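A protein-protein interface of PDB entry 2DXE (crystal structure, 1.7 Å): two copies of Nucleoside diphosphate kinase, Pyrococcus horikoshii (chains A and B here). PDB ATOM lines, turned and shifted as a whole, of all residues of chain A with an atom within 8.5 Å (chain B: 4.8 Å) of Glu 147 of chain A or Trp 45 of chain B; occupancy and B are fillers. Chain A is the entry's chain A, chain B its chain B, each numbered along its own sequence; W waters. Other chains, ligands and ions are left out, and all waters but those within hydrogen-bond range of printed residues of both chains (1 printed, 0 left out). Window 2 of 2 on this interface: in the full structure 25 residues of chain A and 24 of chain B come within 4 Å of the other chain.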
ATOM      1  N   ARG A   9     -13.622  21.331   1.747  1.00  0.00           N
ATOM      2  CA  ARG A   9     -13.938  22.608   2.368  1.00  0.00           C
ATOM      3  C   ARG A   9     -12.731  23.007   3.194  1.00  0.00           C
ATOM      4  O   ARG A   9     -12.095  22.157   3.824  1.00  0.00           O
ATOM      5  CB  ARG A   9     -15.157  22.498   3.282  1.00  0.00           C
ATOM      6  CG  ARG A   9     -16.484  22.409   2.550  1.00  0.00           C
ATOM      7  CD  ARG A   9     -17.636  22.385   3.542  1.00  0.00           C
ATOM      8  NE  ARG A   9     -18.938  22.480   2.888  1.00  0.00           N
ATOM      9  CZ  ARG A   9     -20.098  22.488   3.537  1.00  0.00           C
ATOM     10  NH1 ARG A   9     -20.117  22.405   4.863  1.00  0.00           N
ATOM     11  NH2 ARG A   9     -21.236  22.579   2.864  1.00  0.00           N
ATOM     12  N   LYS A  37     -16.209  28.324  -3.989  1.00  0.00           N
ATOM     13  CA  LYS A  37     -17.517  28.738  -3.488  1.00  0.00           C
ATOM     14  C   LYS A  37     -17.508  29.095  -2.005  1.00  0.00           C
ATOM     15  O   LYS A  37     -16.993  28.341  -1.184  1.00  0.00           O
ATOM     16  CB  LYS A  37     -18.529  27.613  -3.726  1.00  0.00           C
ATOM     17  CG  LYS A  37     -19.950  27.918  -3.276  1.00  0.00           C
ATOM     18  CD  LYS A  37     -20.863  26.715  -3.523  1.00  0.00           C
ATOM     19  CE  LYS A  37     -21.017  26.426  -5.011  1.00  0.00           C
ATOM     20  NZ  LYS A  37     -21.720  25.137  -5.277  1.00  0.00           N
ATOM     21  N   ILE A  38     -18.065  30.254  -1.662  1.00  0.00           N
ATOM     22  CA  ILE A  38     -18.139  30.661  -0.262  1.00  0.00           C
ATOM     23  C   ILE A  38     -19.396  30.007   0.302  1.00  0.00           C
ATOM     24  O   ILE A  38     -20.509  30.387  -0.053  1.00  0.00           O
ATOM     25  CB  ILE A  38     -18.267  32.190  -0.120  1.00  0.00           C
ATOM     26  CG1 ILE A  38     -17.040  32.867  -0.729  1.00  0.00           C
ATOM     27  CG2 ILE A  38     -18.422  32.571   1.351  1.00  0.00           C
ATOM     28  CD1 ILE A  38     -17.161  34.373  -0.833  1.00  0.00           C
ATOM     29  N   VAL A  39     -19.225  29.019   1.175  1.00  0.00           N
ATOM     30  CA  VAL A  39     -20.381  28.338   1.746  1.00  0.00           C
ATOM     31  C   VAL A  39     -20.694  28.804   3.158  1.00  0.00           C
ATOM     32  O   VAL A  39     -21.715  28.428   3.735  1.00  0.00           O
ATOM     33  CB  VAL A  39     -20.198  26.805   1.718  1.00  0.00           C
ATOM     34  CG1 VAL A  39     -20.062  26.340   0.266  1.00  0.00           C
ATOM     35  CG2 VAL A  39     -18.980  26.394   2.530  1.00  0.00           C
ATOM     36  N   GLY A  40     -19.819  29.641   3.705  1.00  0.00           N
ATOM     37  CA  GLY A  40     -20.035  30.174   5.039  1.00  0.00           C
ATOM     38  C   GLY A  40     -19.159  31.390   5.238  1.00  0.00           C
ATOM     39  O   GLY A  40     -18.044  31.427   4.726  1.00  0.00           O
ATOM     40  N   GLU A  82     -15.354  26.171  -0.554  1.00  0.00           N
ATOM     41  CA  GLU A  82     -15.584  24.826  -1.060  1.00  0.00           C
ATOM     42  C   GLU A  82     -15.182  24.716  -2.522  1.00  0.00           C
ATOM     43  O   GLU A  82     -15.427  25.627  -3.315  1.00  0.00           O
ATOM     44  CB  GLU A  82     -17.062  24.465  -0.899  1.00  0.00           C
ATOM     45  CG  GLU A  82     -17.407  23.028  -1.227  1.00  0.00           C
ATOM     46  CD  GLU A  82     -18.839  22.687  -0.858  1.00  0.00           C
ATOM     47  OE1 GLU A  82     -19.766  23.171  -1.542  1.00  0.00           O
ATOM     48  OE2 GLU A  82     -19.036  21.943   0.125  1.00  0.00           O
ATOM     49  N   PRO A 142     -23.531  24.029  11.884  1.00  0.00           N
ATOM     50  CA  PRO A 142     -24.025  23.508  10.604  1.00  0.00           C
ATOM     51  C   PRO A 142     -25.002  24.447   9.897  1.00  0.00           C
ATOM     52  O   PRO A 142     -25.023  24.523   8.670  1.00  0.00           O
ATOM     53  CB  PRO A 142     -24.679  22.190  11.005  1.00  0.00           C
ATOM     54  CG  PRO A 142     -23.829  21.741  12.152  1.00  0.00           C
ATOM     55  CD  PRO A 142     -23.667  23.017  12.946  1.00  0.00           C
ATOM     56  N   GLU A 143     -25.802  25.160  10.683  1.00  0.00           N
ATOM     57  CA  GLU A 143     -26.801  26.081  10.153  1.00  0.00           C
ATOM     58  C   GLU A 143     -26.219  27.326   9.486  1.00  0.00           C
ATOM     59  O   GLU A 143     -26.952  28.094   8.862  1.00  0.00           O
ATOM     60  CB  GLU A 143     -27.749  26.506  11.273  1.00  0.00           C
ATOM     61  CG  GLU A 143     -27.080  27.335  12.352  1.00  0.00           C
ATOM     62  CD  GLU A 143     -27.922  27.449  13.604  1.00  0.00           C
ATOM     63  OE1 GLU A 143     -28.091  26.427  14.302  1.00  0.00           O
ATOM     64  OE2 GLU A 143     -28.417  28.560  13.886  1.00  0.00           O
ATOM     65  N   GLU A 144     -24.910  27.524   9.621  1.00  0.00           N
ATOM     66  CA  GLU A 144     -24.242  28.680   9.027  1.00  0.00           C
ATOM     67  C   GLU A 144     -23.496  28.300   7.751  1.00  0.00           C
ATOM     68  O   GLU A 144     -22.828  29.138   7.142  1.00  0.00           O
ATOM     69  CB  GLU A 144     -23.257  29.290  10.028  1.00  0.00           C
ATOM     70  CG  GLU A 144     -23.912  29.862  11.279  1.00  0.00           C
ATOM     71  CD  GLU A 144     -22.898  30.298  12.318  1.00  0.00           C
ATOM     72  OE1 GLU A 144     -22.299  29.421  12.976  1.00  0.00           O
ATOM     73  OE2 GLU A 144     -22.693  31.518  12.469  1.00  0.00           O
ATOM     74  N   LEU A 145     -23.601  27.035   7.358  1.00  0.00           N
ATOM     75  CA  LEU A 145     -22.932  26.541   6.154  1.00  0.00           C
ATOM     76  C   LEU A 145     -24.003  26.149   5.147  1.00  0.00           C
ATOM     77  O   LEU A 145     -24.971  25.464   5.495  1.00  0.00           O
ATOM     78  CB  LEU A 145     -22.046  25.341   6.494  1.00  0.00           C
ATOM     79  CG  LEU A 145     -20.989  25.629   7.566  1.00  0.00           C
ATOM     80  CD1 LEU A 145     -20.184  24.368   7.843  1.00  0.00           C
ATOM     81  CD2 LEU A 145     -20.075  26.762   7.106  1.00  0.00           C
ATOM     82  N   PHE A 146     -23.821  26.563   3.896  1.00  0.00           N
ATOM     83  CA  PHE A 146     -24.831  26.303   2.882  1.00  0.00           C
ATOM     84  C   PHE A 146     -24.419  25.546   1.630  1.00  0.00           C
ATOM     85  O   PHE A 146     -23.251  25.524   1.237  1.00  0.00           O
ATOM     86  CB  PHE A 146     -25.474  27.632   2.469  1.00  0.00           C
ATOM     87  CG  PHE A 146     -25.811  28.527   3.627  1.00  0.00           C
ATOM     88  CD1 PHE A 146     -24.959  29.569   3.989  1.00  0.00           C
ATOM     89  CD2 PHE A 146     -26.966  28.315   4.376  1.00  0.00           C
ATOM     90  CE1 PHE A 146     -25.253  30.386   5.083  1.00  0.00           C
ATOM     91  CE2 PHE A 146     -27.269  29.127   5.472  1.00  0.00           C
ATOM     92  CZ  PHE A 146     -26.411  30.164   5.826  1.00  0.00           C
ATOM     93  N   GLU A 147     -25.417  24.920   1.016  1.00  0.00           N
ATOM     94  CA  GLU A 147     -25.251  24.166  -0.215  1.00  0.00           C
ATOM     95  C   GLU A 147     -26.126  24.872  -1.247  1.00  0.00           C
ATOM     96  O   GLU A 147     -27.349  24.899  -1.118  1.00  0.00           O
ATOM     97  CB  GLU A 147     -25.732  22.728  -0.018  1.00  0.00           C
ATOM     98  CG  GLU A 147     -25.507  21.821  -1.207  1.00  0.00           C
ATOM     99  CD  GLU A 147     -25.920  20.390  -0.923  1.00  0.00           C
ATOM    100  OE1 GLU A 147     -25.417  19.816   0.064  1.00  0.00           O
ATOM    101  OE2 GLU A 147     -26.744  19.839  -1.685  1.00  0.00           O
ATOM    102  N   TYR A 148     -25.498  25.455  -2.259  1.00  0.00           N
ATOM    103  CA  TYR A 148     -26.241  26.174  -3.286  1.00  0.00           C
ATOM    104  C   TYR A 148     -25.407  26.228  -4.558  1.00  0.00           C
ATOM    105  O   TYR A 148     -24.196  26.020  -4.528  1.00  0.00           O
ATOM    106  CB  TYR A 148     -26.559  27.589  -2.803  1.00  0.00           C
ATOM    107  CG  TYR A 148     -25.339  28.469  -2.663  1.00  0.00           C
ATOM    108  CD1 TYR A 148     -24.939  29.310  -3.701  1.00  0.00           C
ATOM    109  CD2 TYR A 148     -24.566  28.436  -1.505  1.00  0.00           C
ATOM    110  CE1 TYR A 148     -23.793  30.095  -3.591  1.00  0.00           C
ATOM    111  CE2 TYR A 148     -23.417  29.220  -1.381  1.00  0.00           C
ATOM    112  CZ  TYR A 148     -23.037  30.046  -2.429  1.00  0.00           C
ATOM    113  OH  TYR A 148     -21.897  30.817  -2.318  1.00  0.00           O
ATOM    114  N   PRO A 149     -26.045  26.520  -5.694  1.00  0.00           N
ATOM    115  CA  PRO A 149     -25.291  26.579  -6.943  1.00  0.00           C
ATOM    116  C   PRO A 149     -24.686  27.931  -7.293  1.00  0.00           C
ATOM    117  O   PRO A 149     -25.329  28.970  -7.152  1.00  0.00           O
ATOM    118  CB  PRO A 149     -26.328  26.155  -7.975  1.00  0.00           C
ATOM    119  CG  PRO A 149     -27.551  26.832  -7.460  1.00  0.00           C
ATOM    120  CD  PRO A 149     -27.495  26.542  -5.960  1.00  0.00           C
ATOM    121  N   ARG A 150     -23.436  27.904  -7.736  1.00  0.00           N
ATOM    122  CA  ARG A 150     -22.785  29.112  -8.194  1.00  0.00           C
ATOM    123  C   ARG A 150     -23.146  29.103  -9.676  1.00  0.00           C
ATOM    124  O   ARG A 150     -23.522  28.060 -10.216  1.00  0.00           O
ATOM    125  CB  ARG A 150     -21.273  29.040  -7.973  1.00  0.00           C
ATOM    126  CG  ARG A 150     -20.823  29.774  -6.708  1.00  0.00           C
ATOM    127  CD  ARG A 150     -20.738  31.278  -6.962  1.00  0.00           C
ATOM    128  NE  ARG A 150     -19.627  31.576  -7.861  1.00  0.00           N
ATOM    129  CZ  ARG A 150     -18.360  31.679  -7.468  1.00  0.00           C
ATOM    130  NH1 ARG A 150     -18.044  31.528  -6.187  1.00  0.00           N
ATOM    131  NH2 ARG A 150     -17.402  31.885  -8.359  1.00  0.00           N
ATOM    132  N   ASP A 153     -21.680  26.211 -12.014  1.00  0.00           N
ATOM    133  CA  ASP A 153     -21.686  24.826 -11.549  1.00  0.00           C
ATOM    134  C   ASP A 153     -22.161  23.824 -12.600  1.00  0.00           C
ATOM    135  O   ASP A 153     -21.549  22.770 -12.771  1.00  0.00           O
ATOM    136  CB  ASP A 153     -22.543  24.681 -10.292  1.00  0.00           C
ATOM    137  CG  ASP A 153     -21.868  25.244  -9.048  1.00  0.00           C
ATOM    138  OD1 ASP A 153     -20.761  25.818  -9.161  1.00  0.00           O
ATOM    139  OD2 ASP A 153     -22.452  25.110  -7.953  1.00  0.00           O
ATOM    140  N   MET B  43     -22.932  35.652   5.871  1.00  0.00           N
ATOM    141  CA  MET B  43     -23.665  35.006   4.799  1.00  0.00           C
ATOM    142  C   MET B  43     -24.790  34.244   5.492  1.00  0.00           C
ATOM    143  O   MET B  43     -24.553  33.484   6.436  1.00  0.00           O
ATOM    144  CB  MET B  43     -22.786  34.020   4.027  1.00  0.00           C
ATOM    145  CG  MET B  43     -23.568  33.214   2.990  1.00  0.00           C
ATOM    146  SD  MET B  43     -22.551  32.108   1.990  1.00  0.00           S
ATOM    147  CE  MET B  43     -21.949  33.272   0.734  1.00  0.00           C
ATOM    148  N   ILE B  44     -26.014  34.476   5.039  1.00  0.00           N
ATOM    149  CA  ILE B  44     -27.183  33.811   5.595  1.00  0.00           C
ATOM    150  C   ILE B  44     -28.081  33.427   4.434  1.00  0.00           C
ATOM    151  O   ILE B  44     -27.884  33.895   3.313  1.00  0.00           O
ATOM    152  CB  ILE B  44     -27.992  34.751   6.524  1.00  0.00           C
ATOM    153  CG1 ILE B  44     -28.471  35.974   5.735  1.00  0.00           C
ATOM    154  CG2 ILE B  44     -27.140  35.178   7.716  1.00  0.00           C
ATOM    155  CD1 ILE B  44     -29.432  36.871   6.503  1.00  0.00           C
ATOM    156  N   TRP B  45     -29.051  32.556   4.690  1.00  0.00           N
ATOM    157  CA  TRP B  45     -29.997  32.186   3.649  1.00  0.00           C
ATOM    158  C   TRP B  45     -31.339  32.657   4.192  1.00  0.00           C
ATOM    159  O   TRP B  45     -31.899  32.052   5.104  1.00  0.00           O
ATOM    160  CB  TRP B  45     -30.018  30.675   3.410  1.00  0.00           C
ATOM    161  CG  TRP B  45     -30.614  30.306   2.075  1.00  0.00           C
ATOM    162  CD1 TRP B  45     -31.610  30.970   1.403  1.00  0.00           C
ATOM    163  CD2 TRP B  45     -30.242  29.201   1.246  1.00  0.00           C
ATOM    164  NE1 TRP B  45     -31.873  30.345   0.207  1.00  0.00           N
ATOM    165  CE2 TRP B  45     -31.048  29.258   0.085  1.00  0.00           C
ATOM    166  CE3 TRP B  45     -29.304  28.166   1.369  1.00  0.00           C
ATOM    167  CZ2 TRP B  45     -30.942  28.317  -0.950  1.00  0.00           C
ATOM    168  CZ3 TRP B  45     -29.200  27.231   0.340  1.00  0.00           C
ATOM    169  CH2 TRP B  45     -30.016  27.316  -0.804  1.00  0.00           C
ATOM    170  N   ILE B  46     -31.834  33.761   3.642  1.00  0.00           N
ATOM    171  CA  ILE B  46     -33.093  34.347   4.081  1.00  0.00           C
ATOM    172  C   ILE B  46     -34.301  33.456   3.813  1.00  0.00           C
ATOM    173  O   ILE B  46     -34.447  32.898   2.728  1.00  0.00           O
ATOM    174  CB  ILE B  46     -33.309  35.719   3.400  1.00  0.00           C
ATOM    175  CG1 ILE B  46     -32.152  36.653   3.765  1.00  0.00           C
ATOM    176  CG2 ILE B  46     -34.638  36.335   3.833  1.00  0.00           C
ATOM    177  CD1 ILE B  46     -32.196  37.996   3.073  1.00  0.00           C
ATOM    178  N   ASP B  47     -35.156  33.317   4.826  1.00  0.00           N
ATOM    179  CA  ASP B  47     -36.372  32.520   4.709  1.00  0.00           C
ATOM    180  C   ASP B  47     -37.500  33.473   4.333  1.00  0.00           C
ATOM    181  O   ASP B  47     -37.359  34.691   4.468  1.00  0.00           O
ATOM    182  CB  ASP B  47     -36.685  31.826   6.040  1.00  0.00           C
ATOM    183  CG  ASP B  47     -36.910  32.811   7.170  1.00  0.00           C
ATOM    184  OD1 ASP B  47     -37.920  33.542   7.136  1.00  0.00           O
ATOM    185  OD2 ASP B  47     -36.072  32.858   8.094  1.00  0.00           O
ATOM    186  N   THR B  72     -34.695  35.128  -1.662  1.00  0.00           N
ATOM    187  CA  THR B  72     -34.492  33.882  -0.923  1.00  0.00           C
ATOM    188  C   THR B  72     -33.994  32.747  -1.817  1.00  0.00           C
ATOM    189  O   THR B  72     -33.921  31.595  -1.384  1.00  0.00           O
ATOM    190  CB  THR B  72     -35.802  33.405  -0.253  1.00  0.00           C
ATOM    191  OG1 THR B  72     -36.741  33.015  -1.265  1.00  0.00           O
ATOM    192  CG2 THR B  72     -36.414  34.520   0.590  1.00  0.00           C
ATOM    193  N   LYS B  73     -33.638  33.069  -3.058  1.00  0.00           N
ATOM    194  CA  LYS B  73     -33.197  32.051  -4.006  1.00  0.00           C
ATOM    195  C   LYS B  73     -31.939  31.285  -3.603  1.00  0.00           C
ATOM    196  O   LYS B  73     -31.867  30.067  -3.780  1.00  0.00           O
ATOM    197  CB  LYS B  73     -33.015  32.671  -5.394  1.00  0.00           C
ATOM    198  CG  LYS B  73     -32.911  31.646  -6.513  1.00  0.00           C
ATOM    199  CD  LYS B  73     -32.969  32.317  -7.884  1.00  0.00           C
ATOM    200  CE  LYS B  73     -32.886  31.298  -9.010  1.00  0.00           C
ATOM    201  NZ  LYS B  73     -34.036  30.349  -9.010  1.00  0.00           N
ATOM    202  N   THR B  74     -30.945  31.998  -3.082  1.00  0.00           N
ATOM    203  CA  THR B  74     -29.699  31.383  -2.627  1.00  0.00           C
ATOM    204  C   THR B  74     -29.235  32.205  -1.435  1.00  0.00           C
ATOM    205  O   THR B  74     -29.884  33.183  -1.056  1.00  0.00           O
ATOM    206  CB  THR B  74     -28.564  31.443  -3.695  1.00  0.00           C
ATOM    207  OG1 THR B  74     -28.060  32.786  -3.793  1.00  0.00           O
ATOM    208  CG2 THR B  74     -29.072  30.998  -5.056  1.00  0.00           C
ATOM    209  N   PRO B  75     -28.122  31.804  -0.801  1.00  0.00           N
ATOM    210  CA  PRO B  75     -27.672  32.610   0.334  1.00  0.00           C
ATOM    211  C   PRO B  75     -27.285  34.005  -0.156  1.00  0.00           C
ATOM    212  O   PRO B  75     -26.992  34.202  -1.338  1.00  0.00           O
ATOM    213  CB  PRO B  75     -26.456  31.840   0.842  1.00  0.00           C
ATOM    214  CG  PRO B  75     -26.810  30.423   0.539  1.00  0.00           C
ATOM    215  CD  PRO B  75     -27.402  30.519  -0.852  1.00  0.00           C
HETATM  216  O   HOH W   1     -22.238  31.767   7.073  1.00  0.00           O
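The backbone carbonyl oxygen of Ile 38 of chain A lies close to the side-chain sulfur of Met 43 of chain B (3.4 Å).
NE1 of Trp 45 of chain B lies within hydrogen-bond range of O of Thr 72 of chain B (2.9 Å). The side-chain amino group (NZ) of Lys 37 of chain A lies within hydrogen-bond range of the backbone carbonyl oxygen (O) of Tyr 148 of chain A (2.7 Å). The backbone carbonyl oxygen (O) of Ile 38 of chain A lies within hydrogen-bond range of the side-chain hydroxyl (OH) of Tyr 148 of chain A (2.7 Å). The backbone NH of Phe 146 of chain A lies within hydrogen-bond range of the backbone carbonyl oxygen of Val 39 of chain A, at 2.8 Å.
Val 39 of chain A touches Met 43 of chain B (C to SD, 3.97 Å). Met 43 of chain B touches Phe 146 of chain A (O to CE1, 3.5 Å). Phe 146 of chain A touches Ile 44 of chain B (CZ to CA, 3.7 Å). N of Trp 45 of chain B touches CZ of Phe 146 of chain A, at 3.7 Å. Phe 146 of chain A touches Pro 75 of chain B (CB to CG, 3.6 Å). Glu 147 of chain A touches Trp 45 of chain B. Tyr 148 of chain A touches Met 43 of chain B. CG of Tyr 148 of chain A touches CD of Pro 75 of chain B, 3.4 Å away.
Of chain B, only Trp 45 comes within 4 Å of Glu 147 of chain A. Of the printed residues of chain A, Met 43 of chain B touches Ile 38, Val 39, Phe 146 and Tyr 148. Of the printed residues of chain B, Phe 146 of chain A touches Met 43 (3.5 Å), Ile 44 (3.7 Å), Trp 45 (3.7 Å) and Pro 75 (3.6 Å). Of the printed residues of chain B, Ile 38 of chain A touches Met 43 (3.3 Å). Of the printed residues of chain A, Ile 44 of chain B touches Phe 146 (3.7 Å). Glu 82 of chain A touches none of the printed residues of chain B. The nearest printed residue of chain B that does not touch Glu 147 of chain A is Pro 75 of chain B (5.6 Å). The nearest printed residue of chain A that does not touch Trp 45 of chain B is Tyr 148 of chain A (4.003 Å).
Of the 16 printed residues of chain A, 5 touch a printed residue of chain B. Hydrophobic or aromatic side chains of chain A that line the printed part of chain B: Ile 38, Phe 146 and Tyr 148. Hydrophobic or aromatic side chains of chain B that line the printed part of chain A: Met 43, Trp 45 and Pro 75.
No position is printed for both chains. Of the 9 pairs that touch across the chains among the printed residues, none has its exchanged pair printed and touching as well.
Water W1 lies within hydrogen-bond range of O of Glu 144 of chain A (2.7 Å) and O of Met 43 of chain B (3.0 Å).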
